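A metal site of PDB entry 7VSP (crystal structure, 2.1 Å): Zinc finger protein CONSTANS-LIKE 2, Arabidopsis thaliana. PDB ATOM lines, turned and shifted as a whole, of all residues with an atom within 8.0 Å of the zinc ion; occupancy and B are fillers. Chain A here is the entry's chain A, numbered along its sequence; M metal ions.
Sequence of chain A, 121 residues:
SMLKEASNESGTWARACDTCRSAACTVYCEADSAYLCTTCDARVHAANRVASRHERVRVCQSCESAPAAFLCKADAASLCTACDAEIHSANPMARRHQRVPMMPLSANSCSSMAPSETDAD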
ATOM      1  N   TYR A  28       2.593  16.463   3.378  1.00  0.00           N
ATOM      2  CA  TYR A  28       3.179  15.547   2.406  1.00  0.00           C
ATOM      3  C   TYR A  28       4.373  16.241   1.768  1.00  0.00           C
ATOM      4  O   TYR A  28       4.275  17.401   1.369  1.00  0.00           O
ATOM      5  CB  TYR A  28       2.190  15.147   1.293  1.00  0.00           C
ATOM      6  CG  TYR A  28       2.838  14.284   0.212  1.00  0.00           C
ATOM      7  CD1 TYR A  28       3.092  12.930   0.435  1.00  0.00           C
ATOM      8  CD2 TYR A  28       3.241  14.836  -1.006  1.00  0.00           C
ATOM      9  CE1 TYR A  28       3.691  12.149  -0.524  1.00  0.00           C
ATOM     10  CE2 TYR A  28       3.811  14.047  -2.007  1.00  0.00           C
ATOM     11  CZ  TYR A  28       4.042  12.711  -1.742  1.00  0.00           C
ATOM     12  OH  TYR A  28       4.650  11.927  -2.704  1.00  0.00           O
ATOM     13  N   CYS A  29       5.487  15.514   1.670  1.00  0.00           N
ATOM     14  CA  CYS A  29       6.697  16.025   1.027  1.00  0.00           C
ATOM     15  C   CYS A  29       6.970  15.222  -0.228  1.00  0.00           C
ATOM     16  O   CYS A  29       7.281  14.028  -0.152  1.00  0.00           O
ATOM     17  CB  CYS A  29       7.888  15.967   1.971  1.00  0.00           C
ATOM     18  SG  CYS A  29       9.306  16.645   1.120  1.00  0.00           S
ATOM     19  N   GLU A  30       6.862  15.852  -1.377  1.00  0.00           N
ATOM     20  CA  GLU A  30       7.149  15.135  -2.621  1.00  0.00           C
ATOM     21  C   GLU A  30       8.600  14.666  -2.696  1.00  0.00           C
ATOM     22  O   GLU A  30       8.877  13.523  -3.100  1.00  0.00           O
ATOM     23  CB  GLU A  30       6.789  16.004  -3.826  1.00  0.00           C
ATOM     24  CG  GLU A  30       6.951  15.280  -5.159  1.00  0.00           C
ATOM     25  CD  GLU A  30       5.900  14.203  -5.392  1.00  0.00           C
ATOM     26  OE1 GLU A  30       6.059  13.057  -4.871  1.00  0.00           O
ATOM     27  OE2 GLU A  30       4.912  14.487  -6.112  1.00  0.00           O
ATOM     28  N   ALA A  31       9.563  15.523  -2.306  1.00  0.00           N
ATOM     29  CA  ALA A  31      10.981  15.174  -2.448  1.00  0.00           C
ATOM     30  C   ALA A  31      11.320  13.933  -1.656  1.00  0.00           C
ATOM     31  O   ALA A  31      12.128  13.105  -2.097  1.00  0.00           O
ATOM     32  CB  ALA A  31      11.869  16.345  -2.012  1.00  0.00           C
ATOM     33  N   ASP A  32      10.730  13.788  -0.465  1.00  0.00           N
ATOM     34  CA  ASP A  32      10.864  12.632   0.385  1.00  0.00           C
ATOM     35  C   ASP A  32       9.819  11.566   0.094  1.00  0.00           C
ATOM     36  O   ASP A  32       9.954  10.436   0.595  1.00  0.00           O
ATOM     37  CB  ASP A  32      10.749  13.033   1.865  1.00  0.00           C
ATOM     38  CG  ASP A  32      11.990  13.777   2.371  1.00  0.00           C
ATOM     39  OD1 ASP A  32      13.097  13.282   2.086  1.00  0.00           O
ATOM     40  OD2 ASP A  32      11.855  14.824   3.031  1.00  0.00           O
ATOM     41  N   SER A  33       8.802  11.885  -0.715  1.00  0.00           N
ATOM     42  CA  SER A  33       7.710  10.954  -0.972  1.00  0.00           C
ATOM     43  C   SER A  33       7.167  10.410   0.354  1.00  0.00           C
ATOM     44  O   SER A  33       7.054   9.205   0.555  1.00  0.00           O
ATOM     45  CB  SER A  33       8.146   9.806  -1.884  1.00  0.00           C
ATOM     46  OG  SER A  33       6.994   9.019  -2.217  1.00  0.00           O
ATOM     47  N   ALA A  34       6.872  11.335   1.274  1.00  0.00           N
ATOM     48  CA  ALA A  34       6.602  10.986   2.677  1.00  0.00           C
ATOM     49  C   ALA A  34       5.374  11.720   3.184  1.00  0.00           C
ATOM     50  O   ALA A  34       5.239  12.932   2.978  1.00  0.00           O
ATOM     51  CB  ALA A  34       7.808  11.337   3.559  1.00  0.00           C
ATOM     52  N   LEU A  36       3.880  12.879   6.683  1.00  0.00           N
ATOM     53  CA  LEU A  36       4.483  13.128   7.995  1.00  0.00           C
ATOM     54  C   LEU A  36       3.529  13.893   8.895  1.00  0.00           C
ATOM     55  O   LEU A  36       2.830  14.795   8.431  1.00  0.00           O
ATOM     56  CB  LEU A  36       5.782  13.946   7.872  1.00  0.00           C
ATOM     57  CG  LEU A  36       6.832  13.302   6.947  1.00  0.00           C
ATOM     58  CD1 LEU A  36       7.948  14.263   6.592  1.00  0.00           C
ATOM     59  CD2 LEU A  36       7.387  12.025   7.589  1.00  0.00           C
ATOM     60  N   ASP A  41       7.673  16.145  10.495  1.00  0.00           N
ATOM     61  CA  ASP A  41       7.989  17.080   9.434  1.00  0.00           C
ATOM     62  C   ASP A  41       9.050  18.088   9.870  1.00  0.00           C
ATOM     63  O   ASP A  41       9.990  18.397   9.102  1.00  0.00           O
ATOM     64  CB  ASP A  41       6.720  17.800   9.000  1.00  0.00           C
ATOM     65  CG  ASP A  41       6.976  18.810   7.909  1.00  0.00           C
ATOM     66  OD1 ASP A  41       7.350  18.409   6.784  1.00  0.00           O
ATOM     67  OD2 ASP A  41       6.816  20.015   8.156  1.00  0.00           O
ATOM     68  N   VAL A  44      12.505  16.286  10.243  1.00  0.00           N
ATOM     69  CA  VAL A  44      13.113  15.865   9.000  1.00  0.00           C
ATOM     70  C   VAL A  44      13.718  17.063   8.273  1.00  0.00           C
ATOM     71  O   VAL A  44      14.823  16.992   7.728  1.00  0.00           O
ATOM     72  CB  VAL A  44      12.089  15.114   8.119  1.00  0.00           C
ATOM     73  CG1 VAL A  44      12.592  14.998   6.682  1.00  0.00           C
ATOM     74  CG2 VAL A  44      11.762  13.689   8.733  1.00  0.00           C
ATOM     75  N   HIS A  45      13.043  18.201   8.287  1.00  0.00           N
ATOM     76  CA  HIS A  45      13.488  19.317   7.489  1.00  0.00           C
ATOM     77  C   HIS A  45      14.349  20.325   8.257  1.00  0.00           C
ATOM     78  O   HIS A  45      14.883  21.241   7.647  1.00  0.00           O
ATOM     79  CB  HIS A  45      12.265  19.968   6.876  1.00  0.00           C
ATOM     80  CG  HIS A  45      11.512  19.015   5.997  1.00  0.00           C
ATOM     81  ND1 HIS A  45      10.362  18.378   6.408  1.00  0.00           N
ATOM     82  CD2 HIS A  45      11.782  18.539   4.755  1.00  0.00           C
ATOM     83  CE1 HIS A  45       9.944  17.572   5.446  1.00  0.00           C
ATOM     84  NE2 HIS A  45      10.779  17.661   4.435  1.00  0.00           N
ATOM     85  N   VAL A  50      19.873  21.673   3.221  1.00  0.00           N
ATOM     86  CA  VAL A  50      19.413  21.010   2.012  1.00  0.00           C
ATOM     87  C   VAL A  50      17.970  20.542   2.201  1.00  0.00           C
ATOM     88  O   VAL A  50      17.088  20.851   1.398  1.00  0.00           O
ATOM     89  CB  VAL A  50      20.334  19.829   1.648  1.00  0.00           C
ATOM     90  CG1 VAL A  50      19.685  18.967   0.578  1.00  0.00           C
ATOM     91  CG2 VAL A  50      21.704  20.390   1.178  1.00  0.00           C
ATOM     92  N   ALA A  51      17.721  19.810   3.286  1.00  0.00           N
ATOM     93  CA  ALA A  51      16.384  19.292   3.542  1.00  0.00           C
ATOM     94  C   ALA A  51      15.412  20.433   3.804  1.00  0.00           C
ATOM     95  O   ALA A  51      14.225  20.315   3.455  1.00  0.00           O
ATOM     96  CB  ALA A  51      16.378  18.315   4.727  1.00  0.00           C
ATOM     97  N   SER A  52      15.902  21.539   4.404  1.00  0.00           N
ATOM     98  CA  SER A  52      15.005  22.614   4.795  1.00  0.00           C
ATOM     99  C   SER A  52      14.422  23.315   3.596  1.00  0.00           C
ATOM    100  O   SER A  52      13.472  24.085   3.758  1.00  0.00           O
ATOM    101  CB  SER A  52      15.734  23.631   5.694  1.00  0.00           C
ATOM    102  OG  SER A  52      16.615  24.440   4.934  1.00  0.00           O
ATOM    103  N   ARG A  53      14.949  23.063   2.414  1.00  0.00           N
ATOM    104  CA  ARG A  53      14.393  23.674   1.232  1.00  0.00           C
ATOM    105  C   ARG A  53      13.229  22.891   0.667  1.00  0.00           C
ATOM    106  O   ARG A  53      12.607  23.348  -0.302  1.00  0.00           O
ATOM    107  CB  ARG A  53      15.502  23.856   0.187  1.00  0.00           C
ATOM    108  CG  ARG A  53      16.581  24.902   0.631  1.00  0.00           C
ATOM    109  CD  ARG A  53      17.917  24.723  -0.098  1.00  0.00           C
ATOM    110  NE  ARG A  53      17.736  24.112  -1.411  1.00  0.00           N
ATOM    111  CZ  ARG A  53      18.632  23.357  -2.036  1.00  0.00           C
ATOM    112  NH1 ARG A  53      19.860  23.198  -1.547  1.00  0.00           N
ATOM    113  NH2 ARG A  53      18.308  22.794  -3.196  1.00  0.00           N
ATOM    114  N   HIS A  54      12.926  21.704   1.211  1.00  0.00           N
ATOM    115  CA  HIS A  54      11.821  20.902   0.673  1.00  0.00           C
ATOM    116  C   HIS A  54      10.518  21.673   0.766  1.00  0.00           C
ATOM    117  O   HIS A  54      10.212  22.229   1.814  1.00  0.00           O
ATOM    118  CB  HIS A  54      11.691  19.565   1.396  1.00  0.00           C
ATOM    119  CG  HIS A  54      12.842  18.642   1.139  1.00  0.00           C
ATOM    120  ND1 HIS A  54      12.915  17.380   1.677  1.00  0.00           N
ATOM    121  CD2 HIS A  54      13.963  18.808   0.406  1.00  0.00           C
ATOM    122  CE1 HIS A  54      14.032  16.788   1.273  1.00  0.00           C
ATOM    123  NE2 HIS A  54      14.687  17.635   0.506  1.00  0.00           N
ATOM    124  N   GLU A  55       9.768  21.714  -0.324  1.00  0.00           N
ATOM    125  CA  GLU A  55       8.415  22.245  -0.333  1.00  0.00           C
ATOM    126  C   GLU A  55       7.439  21.154   0.085  1.00  0.00           C
ATOM    127  O   GLU A  55       7.450  20.057  -0.482  1.00  0.00           O
ATOM    128  CB  GLU A  55       8.035  22.796  -1.717  1.00  0.00           C
ATOM    129  CG  GLU A  55       9.166  23.470  -2.448  1.00  0.00           C
ATOM    130  CD  GLU A  55       9.033  23.389  -3.964  1.00  0.00           C
ATOM    131  OE1 GLU A  55       7.925  23.675  -4.482  1.00  0.00           O
ATOM    132  OE2 GLU A  55      10.039  23.044  -4.641  1.00  0.00           O
ATOM    133  N   ARG A  56       6.602  21.447   1.081  1.00  0.00           N
ATOM    134  CA  ARG A  56       5.608  20.511   1.593  1.00  0.00           C
ATOM    135  C   ARG A  56       4.195  21.081   1.436  1.00  0.00           C
ATOM    136  O   ARG A  56       3.996  22.301   1.361  1.00  0.00           O
ATOM    137  CB  ARG A  56       5.829  20.188   3.075  1.00  0.00           C
ATOM    138  CG  ARG A  56       6.975  19.269   3.316  1.00  0.00           C
ATOM    139  CD  ARG A  56       8.246  20.106   3.610  1.00  0.00           C
ATOM    140  NE  ARG A  56       8.206  20.593   4.981  1.00  0.00           N
ATOM    141  CZ  ARG A  56       9.001  21.539   5.468  1.00  0.00           C
ATOM    142  NH1 ARG A  56       9.817  22.231   4.690  1.00  0.00           N
ATOM    143  NH2 ARG A  56       8.986  21.772   6.778  1.00  0.00           N
HETATM  144 ZN    ZN M   1      11.042  16.528   2.528  1.00  0.00          ZN
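Four residues have an atom within 4 Å of the zinc ion: Cys 29, Asp 32, His 45 and His 54.
The zinc ion is bound by OD2 of Asp 32, ND1 of His 54, NE2 of His 45 and SG of Cys 29.
The guanidinium group (NH1) of Arg 56 sits at hydrogen-bond distance from the backbone carbonyl oxygen (O) of His 54 (2.9 Å).
The guanidinium group (NE) of Arg 56 sits at hydrogen-bond distance from a ring nitrogen (ND1) of His 45.
A ring nitrogen (ND1) of His 45 lies within hydrogen-bond range of the backbone carbonyl oxygen (O) of Asp 41 (2.7 Å).
The backbone carbonyl oxygen (O) of His 45 lies close to the backbone NH (N) of Ser 52, 3.4 Å away.
SG of Cys 29 sits close to N of Ala 31.
The backbone NH (N) of Cys 29 lies within hydrogen-bond range of the backbone carbonyl oxygen (O) of Ala 34.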
